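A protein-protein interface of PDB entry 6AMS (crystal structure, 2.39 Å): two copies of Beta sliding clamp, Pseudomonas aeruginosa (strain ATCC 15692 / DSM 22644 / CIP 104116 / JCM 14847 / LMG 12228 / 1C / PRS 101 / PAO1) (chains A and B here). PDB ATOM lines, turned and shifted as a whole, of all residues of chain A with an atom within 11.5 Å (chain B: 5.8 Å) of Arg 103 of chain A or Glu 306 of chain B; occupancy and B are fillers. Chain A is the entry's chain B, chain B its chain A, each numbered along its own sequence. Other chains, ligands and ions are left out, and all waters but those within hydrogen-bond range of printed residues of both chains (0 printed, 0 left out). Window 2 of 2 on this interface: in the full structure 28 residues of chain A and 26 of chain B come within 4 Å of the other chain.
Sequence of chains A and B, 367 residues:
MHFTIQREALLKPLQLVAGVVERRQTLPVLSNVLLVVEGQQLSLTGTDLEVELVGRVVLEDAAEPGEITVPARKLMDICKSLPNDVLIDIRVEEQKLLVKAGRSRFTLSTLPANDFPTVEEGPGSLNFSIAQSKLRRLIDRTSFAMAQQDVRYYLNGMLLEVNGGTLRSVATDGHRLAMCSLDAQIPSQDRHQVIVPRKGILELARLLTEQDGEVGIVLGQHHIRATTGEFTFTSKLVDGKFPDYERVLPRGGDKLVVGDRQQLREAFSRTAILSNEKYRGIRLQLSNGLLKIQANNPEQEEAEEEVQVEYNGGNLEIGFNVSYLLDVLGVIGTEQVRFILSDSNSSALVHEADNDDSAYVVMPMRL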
ATOM      1  N   ILE A  78     -17.631  20.207  -7.943  1.00  0.00           N
ATOM      2  CA  ILE A  78     -16.476  19.601  -7.303  1.00  0.00           C
ATOM      3  C   ILE A  78     -15.781  18.699  -8.326  1.00  0.00           C
ATOM      4  O   ILE A  78     -14.592  18.782  -8.499  1.00  0.00           O
ATOM      5  CB  ILE A  78     -16.865  18.838  -6.029  1.00  0.00           C
ATOM      6  CG1 ILE A  78     -17.278  19.819  -4.941  1.00  0.00           C
ATOM      7  CG2 ILE A  78     -15.699  18.080  -5.487  1.00  0.00           C
ATOM      8  CD1 ILE A  78     -18.098  19.211  -3.823  1.00  0.00           C
ATOM      9  N   SER A  81     -14.015  20.773 -11.134  1.00  0.00           N
ATOM     10  CA  SER A  81     -12.831  21.502 -10.680  1.00  0.00           C
ATOM     11  C   SER A  81     -11.628  20.635 -10.341  1.00  0.00           C
ATOM     12  O   SER A  81     -10.574  21.165 -10.050  1.00  0.00           O
ATOM     13  CB  SER A  81     -13.183  22.299  -9.431  1.00  0.00           C
ATOM     14  OG  SER A  81     -13.445  21.411  -8.346  1.00  0.00           O
ATOM     15  N   LEU A  82     -11.801  19.326 -10.327  1.00  0.00           N
ATOM     16  CA  LEU A  82     -10.710  18.430 -10.001  1.00  0.00           C
ATOM     17  C   LEU A  82      -9.762  18.246 -11.172  1.00  0.00           C
ATOM     18  O   LEU A  82     -10.122  18.486 -12.310  1.00  0.00           O
ATOM     19  CB  LEU A  82     -11.244  17.075  -9.542  1.00  0.00           C
ATOM     20  CG  LEU A  82     -11.830  16.994  -8.138  1.00  0.00           C
ATOM     21  CD1 LEU A  82     -12.590  15.701  -7.939  1.00  0.00           C
ATOM     22  CD2 LEU A  82     -10.745  17.157  -7.092  1.00  0.00           C
ATOM     23  N   PRO A  83      -8.536  17.828 -10.881  1.00  0.00           N
ATOM     24  CA  PRO A  83      -7.482  17.571 -11.862  1.00  0.00           C
ATOM     25  C   PRO A  83      -7.924  16.586 -12.935  1.00  0.00           C
ATOM     26  O   PRO A  83      -8.619  15.626 -12.648  1.00  0.00           O
ATOM     27  CB  PRO A  83      -6.380  16.945 -11.020  1.00  0.00           C
ATOM     28  CG  PRO A  83      -6.588  17.499  -9.661  1.00  0.00           C
ATOM     29  CD  PRO A  83      -8.062  17.675  -9.501  1.00  0.00           C
ATOM     30  N   VAL A  86      -7.990  12.311 -12.855  1.00  0.00           N
ATOM     31  CA  VAL A  86      -7.818  11.838 -11.487  1.00  0.00           C
ATOM     32  C   VAL A  86      -8.879  10.798 -11.112  1.00  0.00           C
ATOM     33  O   VAL A  86      -9.957  10.769 -11.689  1.00  0.00           O
ATOM     34  CB  VAL A  86      -7.856  13.001 -10.481  1.00  0.00           C
ATOM     35  CG1 VAL A  86      -9.291  13.342 -10.114  1.00  0.00           C
ATOM     36  CG2 VAL A  86      -7.059  12.662  -9.235  1.00  0.00           C
ATOM     37  N   LEU A  87      -8.543   9.927 -10.167  1.00  0.00           N
ATOM     38  CA  LEU A  87      -9.470   8.915  -9.699  1.00  0.00           C
ATOM     39  C   LEU A  87     -10.137   9.479  -8.460  1.00  0.00           C
ATOM     40  O   LEU A  87      -9.468   9.985  -7.566  1.00  0.00           O
ATOM     41  CB  LEU A  87      -8.748   7.615  -9.365  1.00  0.00           C
ATOM     42  CG  LEU A  87      -9.659   6.442  -9.000  1.00  0.00           C
ATOM     43  CD1 LEU A  87     -10.402   5.950 -10.229  1.00  0.00           C
ATOM     44  CD2 LEU A  87      -8.878   5.307  -8.361  1.00  0.00           C
ATOM     45  N   ILE A  88     -11.456   9.379  -8.401  1.00  0.00           N
ATOM     46  CA  ILE A  88     -12.206   9.920  -7.287  1.00  0.00           C
ATOM     47  C   ILE A  88     -12.781   8.826  -6.407  1.00  0.00           C
ATOM     48  O   ILE A  88     -13.414   7.895  -6.885  1.00  0.00           O
ATOM     49  CB  ILE A  88     -13.339  10.821  -7.801  1.00  0.00           C
ATOM     50  CG1 ILE A  88     -12.796  11.780  -8.859  1.00  0.00           C
ATOM     51  CG2 ILE A  88     -13.990  11.571  -6.653  1.00  0.00           C
ATOM     52  CD1 ILE A  88     -13.858  12.494  -9.657  1.00  0.00           C
ATOM     53  N   ASP A  89     -12.553   8.954  -5.108  1.00  0.00           N
ATOM     54  CA  ASP A  89     -13.035   7.985  -4.146  1.00  0.00           C
ATOM     55  C   ASP A  89     -14.271   8.549  -3.468  1.00  0.00           C
ATOM     56  O   ASP A  89     -14.230   9.616  -2.871  1.00  0.00           O
ATOM     57  CB  ASP A  89     -11.946   7.713  -3.114  1.00  0.00           C
ATOM     58  CG  ASP A  89     -12.246   6.523  -2.246  1.00  0.00           C
ATOM     59  OD1 ASP A  89     -12.995   6.669  -1.264  1.00  0.00           O
ATOM     60  OD2 ASP A  89     -11.710   5.443  -2.539  1.00  0.00           O
ATOM     61  N   LEU A  98     -18.337  11.533   1.391  1.00  0.00           N
ATOM     62  CA  LEU A  98     -16.932  11.872   1.503  1.00  0.00           C
ATOM     63  C   LEU A  98     -16.293  11.682   0.137  1.00  0.00           C
ATOM     64  O   LEU A  98     -16.214  10.572  -0.372  1.00  0.00           O
ATOM     65  CB  LEU A  98     -16.245  10.980   2.536  1.00  0.00           C
ATOM     66  CG  LEU A  98     -16.337  11.363   4.014  1.00  0.00           C
ATOM     67  CD1 LEU A  98     -17.756  11.706   4.429  1.00  0.00           C
ATOM     68  CD2 LEU A  98     -15.776  10.259   4.893  1.00  0.00           C
ATOM     69  N   VAL A  99     -15.837  12.773  -0.459  1.00  0.00           N
ATOM     70  CA  VAL A  99     -15.218  12.697  -1.771  1.00  0.00           C
ATOM     71  C   VAL A  99     -13.717  12.924  -1.675  1.00  0.00           C
ATOM     72  O   VAL A  99     -13.260  13.920  -1.130  1.00  0.00           O
ATOM     73  CB  VAL A  99     -15.840  13.713  -2.739  1.00  0.00           C
ATOM     74  CG1 VAL A  99     -15.200  13.603  -4.110  1.00  0.00           C
ATOM     75  CG2 VAL A  99     -17.342  13.496  -2.830  1.00  0.00           C
ATOM     76  N   LYS A 100     -12.954  11.986  -2.218  1.00  0.00           N
ATOM     77  CA  LYS A 100     -11.506  12.080  -2.188  1.00  0.00           C
ATOM     78  C   LYS A 100     -10.876  11.930  -3.558  1.00  0.00           C
ATOM     79  O   LYS A 100     -11.265  11.086  -4.350  1.00  0.00           O
ATOM     80  CB  LYS A 100     -10.916  11.028  -1.251  1.00  0.00           C
ATOM     81  CG  LYS A 100     -11.082  11.332   0.222  1.00  0.00           C
ATOM     82  CD  LYS A 100     -10.223  10.402   1.058  1.00  0.00           C
ATOM     83  CE  LYS A 100     -10.590   8.949   0.823  1.00  0.00           C
ATOM     84  NZ  LYS A 100      -9.666   8.018   1.524  1.00  0.00           N
ATOM     85  N   ALA A 101      -9.893  12.775  -3.821  1.00  0.00           N
ATOM     86  CA  ALA A 101      -9.145  12.748  -5.061  1.00  0.00           C
ATOM     87  C   ALA A 101      -7.816  13.445  -4.805  1.00  0.00           C
ATOM     88  O   ALA A 101      -7.772  14.635  -4.525  1.00  0.00           O
ATOM     89  CB  ALA A 101      -9.919  13.434  -6.166  1.00  0.00           C
ATOM     90  N   GLY A 102      -6.728  12.698  -4.899  1.00  0.00           N
ATOM     91  CA  GLY A 102      -5.414  13.246  -4.639  1.00  0.00           C
ATOM     92  C   GLY A 102      -5.346  13.707  -3.199  1.00  0.00           C
ATOM     93  O   GLY A 102      -5.533  12.932  -2.274  1.00  0.00           O
ATOM     94  N   ARG A 103      -5.081  14.991  -3.013  1.00  0.00           N
ATOM     95  CA  ARG A 103      -5.026  15.561  -1.703  1.00  0.00           C
ATOM     96  C   ARG A 103      -6.207  16.438  -1.344  1.00  0.00           C
ATOM     97  O   ARG A 103      -6.157  17.105  -0.371  1.00  0.00           O
ATOM     98  CB  ARG A 103      -3.736  16.303  -1.508  1.00  0.00           C
ATOM     99  CG  ARG A 103      -2.666  15.448  -0.875  1.00  0.00           C
ATOM    100  CD  ARG A 103      -1.772  16.268   0.001  1.00  0.00           C
ATOM    101  NE  ARG A 103      -0.720  16.875  -0.771  1.00  0.00           N
ATOM    102  CZ  ARG A 103       0.388  17.342  -0.242  1.00  0.00           C
ATOM    103  NH1 ARG A 103       0.584  17.250   1.075  1.00  0.00           N
ATOM    104  NH2 ARG A 103       1.299  17.861  -1.041  1.00  0.00           N
ATOM    105  N   SER A 104      -7.258  16.435  -2.137  1.00  0.00           N
ATOM    106  CA  SER A 104      -8.442  17.205  -1.850  1.00  0.00           C
ATOM    107  C   SER A 104      -9.523  16.365  -1.188  1.00  0.00           C
ATOM    108  O   SER A 104      -9.921  15.374  -1.717  1.00  0.00           O
ATOM    109  CB  SER A 104      -9.020  17.716  -3.139  1.00  0.00           C
ATOM    110  OG  SER A 104      -8.334  18.810  -3.652  1.00  0.00           O
ATOM    111  N   ARG A 105     -10.021  16.798  -0.045  1.00  0.00           N
ATOM    112  CA  ARG A 105     -11.088  16.117   0.659  1.00  0.00           C
ATOM    113  C   ARG A 105     -12.311  16.979   0.628  1.00  0.00           C
ATOM    114  O   ARG A 105     -12.228  18.151   0.769  1.00  0.00           O
ATOM    115  CB  ARG A 105     -10.763  15.856   2.120  1.00  0.00           C
ATOM    116  CG  ARG A 105      -9.472  15.178   2.460  1.00  0.00           C
ATOM    117  CD  ARG A 105      -9.432  13.732   2.040  1.00  0.00           C
ATOM    118  NE  ARG A 105      -8.089  13.191   2.138  1.00  0.00           N
ATOM    119  CZ  ARG A 105      -7.266  13.037   1.107  1.00  0.00           C
ATOM    120  NH1 ARG A 105      -6.049  12.557   1.305  1.00  0.00           N
ATOM    121  NH2 ARG A 105      -7.631  13.378  -0.112  1.00  0.00           N
ATOM    122  N   PHE A 106     -13.459  16.382   0.390  1.00  0.00           N
ATOM    123  CA  PHE A 106     -14.718  17.087   0.368  1.00  0.00           C
ATOM    124  C   PHE A 106     -15.754  16.315   1.184  1.00  0.00           C
ATOM    125  O   PHE A 106     -15.761  15.127   1.155  1.00  0.00           O
ATOM    126  CB  PHE A 106     -15.215  17.249  -1.061  1.00  0.00           C
ATOM    127  CG  PHE A 106     -14.304  18.005  -1.976  1.00  0.00           C
ATOM    128  CD1 PHE A 106     -14.465  19.335  -2.156  1.00  0.00           C
ATOM    129  CD2 PHE A 106     -13.347  17.358  -2.721  1.00  0.00           C
ATOM    130  CE1 PHE A 106     -13.672  20.024  -3.012  1.00  0.00           C
ATOM    131  CE2 PHE A 106     -12.522  18.040  -3.563  1.00  0.00           C
ATOM    132  CZ  PHE A 106     -12.695  19.381  -3.719  1.00  0.00           C
ATOM    133  N   THR A 107     -16.604  16.990   1.946  1.00  0.00           N
ATOM    134  CA  THR A 107     -17.651  16.315   2.708  1.00  0.00           C
ATOM    135  C   THR A 107     -18.916  17.036   2.322  1.00  0.00           C
ATOM    136  O   THR A 107     -18.986  18.259   2.519  1.00  0.00           O
ATOM    137  CB  THR A 107     -17.405  16.457   4.225  1.00  0.00           C
ATOM    138  OG1 THR A 107     -16.142  15.901   4.563  1.00  0.00           O
ATOM    139  CG2 THR A 107     -18.486  15.803   5.085  1.00  0.00           C
ATOM    140  N   LEU B 290       4.395  23.929   3.782  1.00  0.00           N
ATOM    141  CA  LEU B 290       3.036  23.409   3.682  1.00  0.00           C
ATOM    142  C   LEU B 290       1.934  24.450   3.941  1.00  0.00           C
ATOM    143  O   LEU B 290       1.964  25.164   4.950  1.00  0.00           O
ATOM    144  CB  LEU B 290       2.883  22.239   4.663  1.00  0.00           C
ATOM    145  CG  LEU B 290       1.599  21.380   4.529  1.00  0.00           C
ATOM    146  CD1 LEU B 290       1.615  20.522   3.267  1.00  0.00           C
ATOM    147  CD2 LEU B 290       1.375  20.512   5.763  1.00  0.00           C
ATOM    148  N   LEU B 291       0.952  24.479   3.034  1.00  0.00           N
ATOM    149  CA  LEU B 291      -0.272  25.279   3.191  1.00  0.00           C
ATOM    150  C   LEU B 291      -1.525  24.406   3.161  1.00  0.00           C
ATOM    151  O   LEU B 291      -1.827  23.741   2.156  1.00  0.00           O
ATOM    152  CB  LEU B 291      -0.361  26.325   2.082  1.00  0.00           C
ATOM    153  CG  LEU B 291      -1.501  27.340   2.145  1.00  0.00           C
ATOM    154  CD1 LEU B 291      -1.367  28.253   3.350  1.00  0.00           C
ATOM    155  CD2 LEU B 291      -1.495  28.130   0.840  1.00  0.00           C
ATOM    156  N   LYS B 292      -2.258  24.417   4.274  1.00  0.00           N
ATOM    157  CA  LYS B 292      -3.532  23.718   4.352  1.00  0.00           C
ATOM    158  C   LYS B 292      -4.621  24.748   4.177  1.00  0.00           C
ATOM    159  O   LYS B 292      -4.654  25.753   4.874  1.00  0.00           O
ATOM    160  CB  LYS B 292      -3.692  23.016   5.697  1.00  0.00           C
ATOM    161  CG  LYS B 292      -2.662  21.944   5.984  1.00  0.00           C
ATOM    162  CD  LYS B 292      -2.895  21.336   7.368  1.00  0.00           C
ATOM    163  CE  LYS B 292      -1.684  20.553   7.849  1.00  0.00           C
ATOM    164  NZ  LYS B 292      -1.722  20.469   9.331  1.00  0.00           N
ATOM    165  N   ILE B 293      -5.514  24.477   3.243  1.00  0.00           N
ATOM    166  CA  ILE B 293      -6.635  25.338   2.965  1.00  0.00           C
ATOM    167  C   ILE B 293      -7.900  24.596   3.353  1.00  0.00           C
ATOM    168  O   ILE B 293      -8.111  23.462   2.953  1.00  0.00           O
ATOM    169  CB  ILE B 293      -6.684  25.688   1.482  1.00  0.00           C
ATOM    170  CG1 ILE B 293      -5.318  26.197   1.035  1.00  0.00           C
ATOM    171  CG2 ILE B 293      -7.770  26.709   1.220  1.00  0.00           C
ATOM    172  CD1 ILE B 293      -5.164  26.287  -0.458  1.00  0.00           C
ATOM    173  N   GLU B 304     -11.109  20.426   2.155  1.00  0.00           N
ATOM    174  CA  GLU B 304      -9.739  20.577   2.654  1.00  0.00           C
ATOM    175  C   GLU B 304      -8.832  20.350   1.475  1.00  0.00           C
ATOM    176  O   GLU B 304      -9.139  19.571   0.581  1.00  0.00           O
ATOM    177  CB  GLU B 304      -9.359  19.552   3.727  1.00  0.00           C
ATOM    178  CG  GLU B 304     -10.216  19.530   4.963  1.00  0.00           C
ATOM    179  CD  GLU B 304     -10.152  18.170   5.693  1.00  0.00           C
ATOM    180  OE1 GLU B 304     -11.112  17.373   5.569  1.00  0.00           O
ATOM    181  OE2 GLU B 304      -9.147  17.895   6.384  1.00  0.00           O
ATOM    182  N   GLU B 305      -7.704  21.023   1.480  1.00  0.00           N
ATOM    183  CA  GLU B 305      -6.713  20.798   0.467  1.00  0.00           C
ATOM    184  C   GLU B 305      -5.355  21.246   0.975  1.00  0.00           C
ATOM    185  O   GLU B 305      -5.245  22.256   1.680  1.00  0.00           O
ATOM    186  CB  GLU B 305      -7.083  21.558  -0.801  1.00  0.00           C
ATOM    187  CG  GLU B 305      -6.062  21.334  -1.917  1.00  0.00           C
ATOM    188  CD  GLU B 305      -6.718  21.257  -3.283  1.00  0.00           C
ATOM    189  OE1 GLU B 305      -7.979  21.263  -3.388  1.00  0.00           O
ATOM    190  OE2 GLU B 305      -5.963  21.167  -4.267  1.00  0.00           O
ATOM    191  N   GLU B 306      -4.334  20.464   0.624  1.00  0.00           N
ATOM    192  CA  GLU B 306      -2.957  20.767   0.996  1.00  0.00           C
ATOM    193  C   GLU B 306      -2.163  21.068  -0.251  1.00  0.00           C
ATOM    194  O   GLU B 306      -2.367  20.430  -1.291  1.00  0.00           O
ATOM    195  CB  GLU B 306      -2.347  19.616   1.789  1.00  0.00           C
ATOM    196  CG  GLU B 306      -3.133  19.301   3.063  1.00  0.00           C
ATOM    197  CD  GLU B 306      -2.372  18.507   4.089  1.00  0.00           C
ATOM    198  OE1 GLU B 306      -1.218  18.125   3.821  1.00  0.00           O
ATOM    199  OE2 GLU B 306      -2.927  18.320   5.194  1.00  0.00           O
ATOM    200  N   VAL B 307      -1.329  22.102  -0.163  1.00  0.00           N
ATOM    201  CA  VAL B 307      -0.439  22.476  -1.247  1.00  0.00           C
ATOM    202  C   VAL B 307       0.949  22.742  -0.663  1.00  0.00           C
ATOM    203  O   VAL B 307       1.107  23.311   0.441  1.00  0.00           O
ATOM    204  CB  VAL B 307      -0.940  23.712  -2.024  1.00  0.00           C
ATOM    205  CG1 VAL B 307       0.005  24.041  -3.179  1.00  0.00           C
ATOM    206  CG2 VAL B 307      -2.372  23.508  -2.530  1.00  0.00           C
ATOM    207  N   GLN B 308       1.984  22.261  -1.342  1.00  0.00           N
ATOM    208  CA  GLN B 308       3.338  22.497  -0.875  1.00  0.00           C
ATOM    209  C   GLN B 308       3.792  23.862  -1.366  1.00  0.00           C
ATOM    210  O   GLN B 308       3.701  24.173  -2.548  1.00  0.00           O
ATOM    211  CB  GLN B 308       4.282  21.392  -1.345  1.00  0.00           C
ATOM    212  CG  GLN B 308       4.152  20.102  -0.555  1.00  0.00           C
ATOM    213  CD  GLN B 308       4.903  18.953  -1.188  1.00  0.00           C
ATOM    214  OE1 GLN B 308       4.860  18.763  -2.397  1.00  0.00           O
ATOM    215  NE2 GLN B 308       5.588  18.175  -0.369  1.00  0.00           N
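The backbone carbonyl oxygen (O) of Arg 105 of chain A sits at hydrogen-bond distance from the backbone NH (N) of Glu 304 of chain B, 2.9 Å away. The side-chain hydroxyl of Ser 104 of chain A lies within hydrogen-bond range of the side-chain carboxylate of Glu 305 of chain B (2.5 Å). The guanidinium group of Arg 103 of chain A lies within salt-bridge range of the side-chain carboxylate of Glu 306 of chain B, 3.4 Å away.
N of Ile 293 of chain B lies within hydrogen-bond range of O of Glu 305 of chain B, 2.7 Å away. O of Gly 102 of chain A sits at hydrogen-bond distance from NH2 of Arg 105 of chain A.
Arg 103 of chain A touches Glu 304 of chain B. Arg 103 of chain A touches Glu 305 of chain B (O to CA, 3.8 Å). NH2 of Arg 103 of chain A touches CG of Gln 308 of chain B (3.7 Å). Ser 104 of chain A touches Glu 304 of chain B (CA to O, 3.5 Å).
Printed residues of chain B within 4 Å of Arg 103 of chain A: Glu 304, Glu 305, Glu 306 and Gln 308. Of the printed residues of chain A, Glu 306 of chain B touches Arg 103 (3.4 Å). No residue of chain A comes within 4 Å of Lys 292 of chain B. No residue of chain A comes within 4 Å of Ile 293 of chain B. Of the printed residues of chain A, Glu 305 of chain B touches Arg 103 (3.8 Å) and Ser 104 (2.5 Å). Gln 308 of chain B touches just one residue of chain A: Arg 103 (3.7 Å). Printed residues of chain A within 4 Å of Glu 304 of chain B: Arg 103, Ser 104 and Arg 105. Of the printed residues of chain B, Ser 104 of chain A touches Glu 304 (3.5 Å) and Glu 305 (2.5 Å). Of the printed residues of chain B, Arg 105 of chain A touches Glu 304.
Of the 18 printed residues of chain A, 3 touch a printed residue of chain B. Along chain A the printed residues that touch a printed residue of chain B span positions 103 to 105.
No position is printed for both chains.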
